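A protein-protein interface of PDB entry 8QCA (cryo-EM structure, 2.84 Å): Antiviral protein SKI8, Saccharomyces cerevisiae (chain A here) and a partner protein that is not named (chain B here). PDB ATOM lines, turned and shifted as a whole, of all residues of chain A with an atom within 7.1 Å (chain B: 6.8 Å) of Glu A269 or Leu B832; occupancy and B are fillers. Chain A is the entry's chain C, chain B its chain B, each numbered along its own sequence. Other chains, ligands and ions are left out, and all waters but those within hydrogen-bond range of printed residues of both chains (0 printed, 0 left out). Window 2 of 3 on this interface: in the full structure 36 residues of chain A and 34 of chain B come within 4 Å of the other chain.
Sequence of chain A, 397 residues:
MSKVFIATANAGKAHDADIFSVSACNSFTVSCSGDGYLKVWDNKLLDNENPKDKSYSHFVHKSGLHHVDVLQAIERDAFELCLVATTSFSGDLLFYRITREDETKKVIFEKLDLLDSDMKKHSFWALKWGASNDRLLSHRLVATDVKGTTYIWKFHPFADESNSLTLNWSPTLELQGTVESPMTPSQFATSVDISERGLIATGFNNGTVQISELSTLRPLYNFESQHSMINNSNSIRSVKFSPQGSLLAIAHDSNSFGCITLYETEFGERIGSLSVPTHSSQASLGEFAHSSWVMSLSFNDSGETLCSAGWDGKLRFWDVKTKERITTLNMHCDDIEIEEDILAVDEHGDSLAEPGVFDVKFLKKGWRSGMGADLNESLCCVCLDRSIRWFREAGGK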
ATOM      1  N   TYR A 221      30.221  -0.511  -7.373  1.00  0.00           N
ATOM      2  CA  TYR A 221      29.508   0.706  -7.023  1.00  0.00           C
ATOM      3  C   TYR A 221      30.407   1.610  -6.194  1.00  0.00           C
ATOM      4  O   TYR A 221      31.363   1.161  -5.559  1.00  0.00           O
ATOM      5  CB  TYR A 221      28.225   0.394  -6.237  1.00  0.00           C
ATOM      6  CG  TYR A 221      27.262  -0.514  -6.964  1.00  0.00           C
ATOM      7  CD1 TYR A 221      27.112  -0.441  -8.341  1.00  0.00           C
ATOM      8  CD2 TYR A 221      26.528  -1.468  -6.276  1.00  0.00           C
ATOM      9  CE1 TYR A 221      26.242  -1.276  -9.010  1.00  0.00           C
ATOM     10  CE2 TYR A 221      25.657  -2.309  -6.936  1.00  0.00           C
ATOM     11  CZ  TYR A 221      25.518  -2.209  -8.302  1.00  0.00           C
ATOM     12  OH  TYR A 221      24.651  -3.044  -8.968  1.00  0.00           O
ATOM     13  N   PHE A 223      29.031   4.836  -3.950  1.00  0.00           N
ATOM     14  CA  PHE A 223      28.036   5.814  -3.541  1.00  0.00           C
ATOM     15  C   PHE A 223      28.510   6.560  -2.303  1.00  0.00           C
ATOM     16  O   PHE A 223      29.227   6.015  -1.459  1.00  0.00           O
ATOM     17  CB  PHE A 223      26.671   5.163  -3.287  1.00  0.00           C
ATOM     18  CG  PHE A 223      26.717   3.945  -2.416  1.00  0.00           C
ATOM     19  CD1 PHE A 223      26.772   4.060  -1.040  1.00  0.00           C
ATOM     20  CD2 PHE A 223      26.679   2.680  -2.975  1.00  0.00           C
ATOM     21  CE1 PHE A 223      26.800   2.938  -0.241  1.00  0.00           C
ATOM     22  CE2 PHE A 223      26.710   1.556  -2.180  1.00  0.00           C
ATOM     23  CZ  PHE A 223      26.771   1.686  -0.811  1.00  0.00           C
ATOM     24  N   LEU A 262      19.985   3.181   4.234  1.00  0.00           N
ATOM     25  CA  LEU A 262      19.739   1.878   3.631  1.00  0.00           C
ATOM     26  C   LEU A 262      19.920   1.956   2.121  1.00  0.00           C
ATOM     27  O   LEU A 262      19.402   2.871   1.474  1.00  0.00           O
ATOM     28  CB  LEU A 262      18.332   1.377   3.964  1.00  0.00           C
ATOM     29  CG  LEU A 262      17.975   1.249   5.445  1.00  0.00           C
ATOM     30  CD1 LEU A 262      16.491   0.972   5.610  1.00  0.00           C
ATOM     31  CD2 LEU A 262      18.800   0.159   6.107  1.00  0.00           C
ATOM     32  N   TYR A 263      20.654   0.992   1.568  1.00  0.00           N
ATOM     33  CA  TYR A 263      20.868   0.870   0.135  1.00  0.00           C
ATOM     34  C   TYR A 263      20.505  -0.540  -0.305  1.00  0.00           C
ATOM     35  O   TYR A 263      20.538  -1.484   0.487  1.00  0.00           O
ATOM     36  CB  TYR A 263      22.324   1.167  -0.251  1.00  0.00           C
ATOM     37  CG  TYR A 263      22.710   2.624  -0.189  1.00  0.00           C
ATOM     38  CD1 TYR A 263      23.029   3.226   1.019  1.00  0.00           C
ATOM     39  CD2 TYR A 263      22.770   3.396  -1.341  1.00  0.00           C
ATOM     40  CE1 TYR A 263      23.389   4.556   1.081  1.00  0.00           C
ATOM     41  CE2 TYR A 263      23.129   4.726  -1.289  1.00  0.00           C
ATOM     42  CZ  TYR A 263      23.437   5.301  -0.076  1.00  0.00           C
ATOM     43  OH  TYR A 263      23.794   6.628  -0.019  1.00  0.00           O
ATOM     44  N   GLU A 264      20.158  -0.682  -1.580  1.00  0.00           N
ATOM     45  CA  GLU A 264      19.907  -1.986  -2.177  1.00  0.00           C
ATOM     46  C   GLU A 264      21.049  -2.308  -3.132  1.00  0.00           C
ATOM     47  O   GLU A 264      21.462  -1.455  -3.922  1.00  0.00           O
ATOM     48  CB  GLU A 264      18.544  -2.025  -2.880  1.00  0.00           C
ATOM     49  CG  GLU A 264      18.342  -1.058  -4.036  1.00  0.00           C
ATOM     50  CD  GLU A 264      18.839  -1.610  -5.357  1.00  0.00           C
ATOM     51  OE1 GLU A 264      18.990  -2.844  -5.466  1.00  0.00           O
ATOM     52  OE2 GLU A 264      19.067  -0.815  -6.290  1.00  0.00           O
ATOM     53  N   THR A 265      21.573  -3.528  -3.036  1.00  0.00           N
ATOM     54  CA  THR A 265      22.850  -3.866  -3.648  1.00  0.00           C
ATOM     55  C   THR A 265      22.739  -4.368  -5.082  1.00  0.00           C
ATOM     56  O   THR A 265      23.773  -4.585  -5.720  1.00  0.00           O
ATOM     57  CB  THR A 265      23.573  -4.921  -2.801  1.00  0.00           C
ATOM     58  OG1 THR A 265      22.723  -6.059  -2.620  1.00  0.00           O
ATOM     59  CG2 THR A 265      23.939  -4.348  -1.444  1.00  0.00           C
ATOM     60  N   GLU A 266      21.528  -4.559  -5.607  1.00  0.00           N
ATOM     61  CA  GLU A 266      21.403  -4.998  -6.993  1.00  0.00           C
ATOM     62  C   GLU A 266      21.799  -3.891  -7.963  1.00  0.00           C
ATOM     63  O   GLU A 266      22.492  -4.146  -8.954  1.00  0.00           O
ATOM     64  CB  GLU A 266      19.980  -5.476  -7.273  1.00  0.00           C
ATOM     65  CG  GLU A 266      19.471  -6.510  -6.286  1.00  0.00           C
ATOM     66  CD  GLU A 266      18.549  -7.525  -6.929  1.00  0.00           C
ATOM     67  OE1 GLU A 266      18.731  -7.817  -8.129  1.00  0.00           O
ATOM     68  OE2 GLU A 266      17.644  -8.033  -6.234  1.00  0.00           O
ATOM     69  N   PHE A 267      21.369  -2.658  -7.696  1.00  0.00           N
ATOM     70  CA  PHE A 267      21.702  -1.522  -8.541  1.00  0.00           C
ATOM     71  C   PHE A 267      22.393  -0.388  -7.801  1.00  0.00           C
ATOM     72  O   PHE A 267      22.899   0.531  -8.454  1.00  0.00           O
ATOM     73  CB  PHE A 267      20.439  -0.975  -9.225  1.00  0.00           C
ATOM     74  N   GLY A 268      22.427  -0.416  -6.472  1.00  0.00           N
ATOM     75  CA  GLY A 268      23.122   0.602  -5.711  1.00  0.00           C
ATOM     76  C   GLY A 268      22.429   1.947  -5.699  1.00  0.00           C
ATOM     77  O   GLY A 268      23.010   2.951  -6.120  1.00  0.00           O
ATOM     78  N   GLU A 269      21.190   1.986  -5.217  1.00  0.00           N
ATOM     79  CA  GLU A 269      20.429   3.221  -5.119  1.00  0.00           C
ATOM     80  C   GLU A 269      20.017   3.462  -3.673  1.00  0.00           C
ATOM     81  O   GLU A 269      19.810   2.522  -2.902  1.00  0.00           O
ATOM     82  CB  GLU A 269      19.187   3.189  -6.017  1.00  0.00           C
ATOM     83  CG  GLU A 269      18.149   2.164  -5.608  1.00  0.00           C
ATOM     84  CD  GLU A 269      16.923   2.189  -6.494  1.00  0.00           C
ATOM     85  OE1 GLU A 269      16.416   3.294  -6.779  1.00  0.00           O
ATOM     86  OE2 GLU A 269      16.467   1.102  -6.906  1.00  0.00           O
ATOM     87  N   ARG A 270      19.909   4.738  -3.313  1.00  0.00           N
ATOM     88  CA  ARG A 270      19.541   5.108  -1.953  1.00  0.00           C
ATOM     89  C   ARG A 270      18.064   4.825  -1.714  1.00  0.00           C
ATOM     90  O   ARG A 270      17.205   5.236  -2.500  1.00  0.00           O
ATOM     91  CB  ARG A 270      19.849   6.585  -1.714  1.00  0.00           C
ATOM     92  CG  ARG A 270      19.779   7.025  -0.265  1.00  0.00           C
ATOM     93  CD  ARG A 270      19.986   8.526  -0.157  1.00  0.00           C
ATOM     94  NE  ARG A 270      19.877   9.010   1.213  1.00  0.00           N
ATOM     95  CZ  ARG A 270      18.734   9.311   1.813  1.00  0.00           C
ATOM     96  NH1 ARG A 270      17.573   9.176   1.195  1.00  0.00           N
ATOM     97  NH2 ARG A 270      18.756   9.759   3.064  1.00  0.00           N
ATOM     98  N   ILE A 271      17.769   4.124  -0.626  1.00  0.00           N
ATOM     99  CA  ILE A 271      16.403   3.743  -0.282  1.00  0.00           C
ATOM    100  C   ILE A 271      15.793   4.701   0.732  1.00  0.00           C
ATOM    101  O   ILE A 271      14.674   5.179   0.551  1.00  0.00           O
ATOM    102  CB  ILE A 271      16.369   2.287   0.231  1.00  0.00           C
ATOM    103  CG1 ILE A 271      16.839   1.329  -0.864  1.00  0.00           C
ATOM    104  CG2 ILE A 271      14.978   1.920   0.716  1.00  0.00           C
ATOM    105  CD1 ILE A 271      16.106   1.497  -2.173  1.00  0.00           C
ATOM    106  N   GLY A 272      16.518   4.994   1.804  1.00  0.00           N
ATOM    107  CA  GLY A 272      16.012   5.892   2.819  1.00  0.00           C
ATOM    108  C   GLY A 272      16.948   5.928   4.009  1.00  0.00           C
ATOM    109  O   GLY A 272      18.077   5.440   3.950  1.00  0.00           O
ATOM    110  N   GLY B 829       9.459   2.910  -4.244  1.00  0.00           N
ATOM    111  CA  GLY B 829      10.642   3.714  -4.467  1.00  0.00           C
ATOM    112  C   GLY B 829      11.842   2.989  -5.033  1.00  0.00           C
ATOM    113  O   GLY B 829      12.939   3.558  -5.031  1.00  0.00           O
ATOM    114  N   PHE B 830      11.678   1.757  -5.509  1.00  0.00           N
ATOM    115  CA  PHE B 830      12.774   1.008  -6.123  1.00  0.00           C
ATOM    116  C   PHE B 830      12.716   1.177  -7.642  1.00  0.00           C
ATOM    117  O   PHE B 830      12.412   0.256  -8.397  1.00  0.00           O
ATOM    118  CB  PHE B 830      12.705  -0.464  -5.722  1.00  0.00           C
ATOM    119  CG  PHE B 830      13.103  -0.735  -4.297  1.00  0.00           C
ATOM    120  CD1 PHE B 830      12.402  -0.175  -3.242  1.00  0.00           C
ATOM    121  CD2 PHE B 830      14.173  -1.563  -4.013  1.00  0.00           C
ATOM    122  CE1 PHE B 830      12.766  -0.430  -1.935  1.00  0.00           C
ATOM    123  CE2 PHE B 830      14.541  -1.822  -2.707  1.00  0.00           C
ATOM    124  CZ  PHE B 830      13.835  -1.255  -1.667  1.00  0.00           C
ATOM    125  N   LEU B 831      13.025   2.397  -8.081  1.00  0.00           N
ATOM    126  CA  LEU B 831      12.869   2.768  -9.481  1.00  0.00           C
ATOM    127  C   LEU B 831      13.913   2.144 -10.399  1.00  0.00           C
ATOM    128  O   LEU B 831      13.722   2.159 -11.619  1.00  0.00           O
ATOM    129  CB  LEU B 831      12.917   4.290  -9.630  1.00  0.00           C
ATOM    130  CG  LEU B 831      12.065   5.123  -8.670  1.00  0.00           C
ATOM    131  CD1 LEU B 831      12.150   6.592  -9.035  1.00  0.00           C
ATOM    132  CD2 LEU B 831      10.622   4.654  -8.678  1.00  0.00           C
ATOM    133  N   LEU B 832      15.004   1.604  -9.860  1.00  0.00           N
ATOM    134  CA  LEU B 832      16.056   1.044 -10.701  1.00  0.00           C
ATOM    135  C   LEU B 832      15.835  -0.423 -11.034  1.00  0.00           C
ATOM    136  O   LEU B 832      16.287  -0.882 -12.090  1.00  0.00           O
ATOM    137  CB  LEU B 832      17.419   1.221 -10.029  1.00  0.00           C
ATOM    138  CG  LEU B 832      18.212   2.447 -10.484  1.00  0.00           C
ATOM    139  CD1 LEU B 832      19.520   2.565  -9.721  1.00  0.00           C
ATOM    140  CD2 LEU B 832      18.466   2.390 -11.980  1.00  0.00           C
ATOM    141  N   LYS B 833      15.163  -1.179 -10.165  1.00  0.00           N
ATOM    142  CA  LYS B 833      14.822  -2.560 -10.478  1.00  0.00           C
ATOM    143  C   LYS B 833      13.466  -2.694 -11.153  1.00  0.00           C
ATOM    144  O   LYS B 833      13.199  -3.729 -11.778  1.00  0.00           O
ATOM    145  CB  LYS B 833      14.850  -3.420  -9.211  1.00  0.00           C
ATOM    146  CG  LYS B 833      16.236  -3.604  -8.597  1.00  0.00           C
ATOM    147  CD  LYS B 833      17.161  -4.431  -9.494  1.00  0.00           C
ATOM    148  CE  LYS B 833      18.158  -3.555 -10.248  1.00  0.00           C
ATOM    149  NZ  LYS B 833      19.061  -4.343 -11.125  1.00  0.00           N
ATOM    150  N   SER B 834      12.616  -1.670 -11.054  1.00  0.00           N
ATOM    151  CA  SER B 834      11.329  -1.706 -11.739  1.00  0.00           C
ATOM    152  C   SER B 834      11.511  -1.765 -13.249  1.00  0.00           C
ATOM    153  O   SER B 834      10.808  -2.512 -13.934  1.00  0.00           O
ATOM    154  CB  SER B 834      10.492  -0.491 -11.346  1.00  0.00           C
ATOM    155  OG  SER B 834      10.128  -0.548  -9.980  1.00  0.00           O
ATOM    156  N   VAL B 835      12.453  -0.989 -13.787  1.00  0.00           N
ATOM    157  CA  VAL B 835      12.682  -1.001 -15.229  1.00  0.00           C
ATOM    158  C   VAL B 835      13.271  -2.335 -15.672  1.00  0.00           C
ATOM    159  O   VAL B 835      12.959  -2.834 -16.759  1.00  0.00           O
ATOM    160  CB  VAL B 835      13.570   0.186 -15.642  1.00  0.00           C
ATOM    161  CG1 VAL B 835      12.778   1.478 -15.586  1.00  0.00           C
ATOM    162  CG2 VAL B 835      14.791   0.277 -14.745  1.00  0.00           C
ATOM    163  N   SER B 836      14.133  -2.934 -14.848  1.00  0.00           N
ATOM    164  CA  SER B 836      14.681  -4.244 -15.189  1.00  0.00           C
ATOM    165  C   SER B 836      13.592  -5.310 -15.210  1.00  0.00           C
ATOM    166  O   SER B 836      13.546  -6.149 -16.121  1.00  0.00           O
ATOM    167  CB  SER B 836      15.786  -4.621 -14.205  1.00  0.00           C
ATOM    168  OG  SER B 836      15.273  -4.737 -12.892  1.00  0.00           O
ATOM    169  N   ILE B 837      12.697  -5.291 -14.222  1.00  0.00           N
ATOM    170  CA  ILE B 837      11.605  -6.260 -14.213  1.00  0.00           C
ATOM    171  C   ILE B 837      10.627  -5.987 -15.352  1.00  0.00           C
ATOM    172  O   ILE B 837      10.045  -6.921 -15.914  1.00  0.00           O
ATOM    173  CB  ILE B 837      10.915  -6.269 -12.838  1.00  0.00           C
ATOM    174  CG1 ILE B 837      11.885  -6.784 -11.777  1.00  0.00           C
ATOM    175  CG2 ILE B 837       9.672  -7.140 -12.856  1.00  0.00           C
ATOM    176  CD1 ILE B 837      11.319  -6.787 -10.391  1.00  0.00           C
ATOM    177  N   ILE B 873       9.501   6.695 -15.603  1.00  0.00           N
ATOM    178  CA  ILE B 873      10.930   6.777 -15.302  1.00  0.00           C
ATOM    179  C   ILE B 873      11.617   7.160 -16.609  1.00  0.00           C
ATOM    180  O   ILE B 873      12.099   6.313 -17.360  1.00  0.00           O
ATOM    181  CB  ILE B 873      11.468   5.477 -14.713  1.00  0.00           C
ATOM    182  CG1 ILE B 873      10.479   4.917 -13.688  1.00  0.00           C
ATOM    183  CG2 ILE B 873      12.824   5.707 -14.067  1.00  0.00           C
ATOM    184  CD1 ILE B 873      10.816   3.530 -13.205  1.00  0.00           C
ATOM    185  N   LYS B 876      15.507   6.584 -17.638  1.00  0.00           N
ATOM    186  CA  LYS B 876      15.875   5.248 -18.088  1.00  0.00           C
ATOM    187  C   LYS B 876      15.031   4.834 -19.287  1.00  0.00           C
ATOM    188  O   LYS B 876      14.737   3.654 -19.485  1.00  0.00           O
ATOM    189  CB  LYS B 876      15.731   4.236 -16.955  1.00  0.00           C
ATOM    190  CG  LYS B 876      16.626   4.498 -15.757  1.00  0.00           C
ATOM    191  CD  LYS B 876      18.085   4.255 -16.089  1.00  0.00           C
ATOM    192  CE  LYS B 876      18.377   2.773 -16.235  1.00  0.00           C
ATOM    193  NZ  LYS B 876      19.816   2.520 -16.506  1.00  0.00           N
ATOM    194  N   GLN B1131      15.894  12.674  -6.149  1.00  0.00           N
ATOM    195  CA  GLN B1131      14.787  11.776  -6.459  1.00  0.00           C
ATOM    196  C   GLN B1131      13.947  12.294  -7.620  1.00  0.00           C
ATOM    197  O   GLN B1131      13.429  11.500  -8.413  1.00  0.00           O
ATOM    198  CB  GLN B1131      13.910  11.572  -5.224  1.00  0.00           C
ATOM    199  CG  GLN B1131      14.541  10.705  -4.152  1.00  0.00           C
ATOM    200  CD  GLN B1131      14.558   9.238  -4.528  1.00  0.00           C
ATOM    201  OE1 GLN B1131      15.609   8.598  -4.531  1.00  0.00           O
ATOM    202  NE2 GLN B1131      13.389   8.697  -4.849  1.00  0.00           N
ATOM    203  N   LYS B1134      15.261  11.537 -11.263  1.00  0.00           N
ATOM    204  CA  LYS B1134      15.159  10.173 -11.766  1.00  0.00           C
ATOM    205  C   LYS B1134      13.917   9.963 -12.620  1.00  0.00           C
ATOM    206  O   LYS B1134      13.898   9.045 -13.446  1.00  0.00           O
ATOM    207  CB  LYS B1134      15.167   9.182 -10.603  1.00  0.00           C
ATOM    208  CG  LYS B1134      16.556   8.765 -10.157  1.00  0.00           C
ATOM    209  CD  LYS B1134      16.496   7.644  -9.136  1.00  0.00           C
ATOM    210  CE  LYS B1134      16.444   8.191  -7.722  1.00  0.00           C
ATOM    211  NZ  LYS B1134      16.877   7.185  -6.716  1.00  0.00           N
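N of Leu B832 lies close to OE2 of Glu A269 (3.3 Å).
The side-chain amino group (NZ) of Lys B1134 is in salt-bridge range of the side-chain carboxylate (OE1) of Glu A269 (3.9 Å).
The side-chain hydroxyl (OG) of Ser B834 is in hydrogen-bond range of the backbone carbonyl oxygen (O) of Phe B830 (2.9 Å).
O of Lys B833 lies within hydrogen-bond range of OG of Ser B836, 2.6 Å away.
The side-chain amide oxygen (OE1) of Gln B1131 sits at hydrogen-bond distance from the side-chain amino group (NZ) of Lys B1134 (2.9 Å).
The side-chain hydroxyl (OH) of Tyr A221 is in hydrogen-bond range of the backbone carbonyl oxygen (O) of Glu A266 (2.4 Å).
O of Leu A262 is in hydrogen-bond range of N of Ile A271 (2.9 Å).
OE1 of Glu A264 sits at hydrogen-bond distance from N of Phe A267 (3.3 Å).
CD of Lys B833 touches CB of Glu A266 (3.7 Å).
Phe A267 touches Leu B832 (CB to CD1, 3.7 Å).
Phe A267 touches Lys B833 (CB to CE, 3.6 Å).
Glu A269 touches Gly B829.
Phe B830 touches Glu A269 (CA to OE2, 3.8 Å).
Leu B831 touches Glu A269.
Phe B830 touches Ile A271 (CZ to CD1, 3.6 Å).
Leu A262 touches none of the printed residues of chain B.
Printed residues of chain B within 4 Å of Glu A266: Lys B833 (3.7 Å).
Of the printed residues of chain B, Phe A267 touches Leu B832 and Lys B833.
Of the printed residues of chain B, Glu A269 touches Gly B829, Phe B830, Leu B831, Leu B832 and Lys B1134.
Printed residues of chain A within 4 Å of Gly B829: Glu A269 (3.9 Å).
Leu B832 touches just these residues of chain A: Phe A267 (3.7 Å) and Glu A269 (3.3 Å).
Printed residues of chain A within 4 Å of Lys B1134: Glu A269 (3.9 Å).
The nearest residue of chain A that does not touch Leu B832 is Glu A264 (4.6 Å).
Of the 13 printed residues of chain A, 4 touch a printed residue of chain B.
Hydrophobic or aromatic side chains of chain A that line the printed part of chain B: Phe A267 and Ile A271.
Along chain A the printed residues that touch a printed residue of chain B span positions 266 to 271.
Among the printed residues, Asp or Glu carboxylates within 4 Å of a Lys or Arg side-chain nitrogen of the other chain: Glu A269 with Lys B1134 (3.9 Å).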
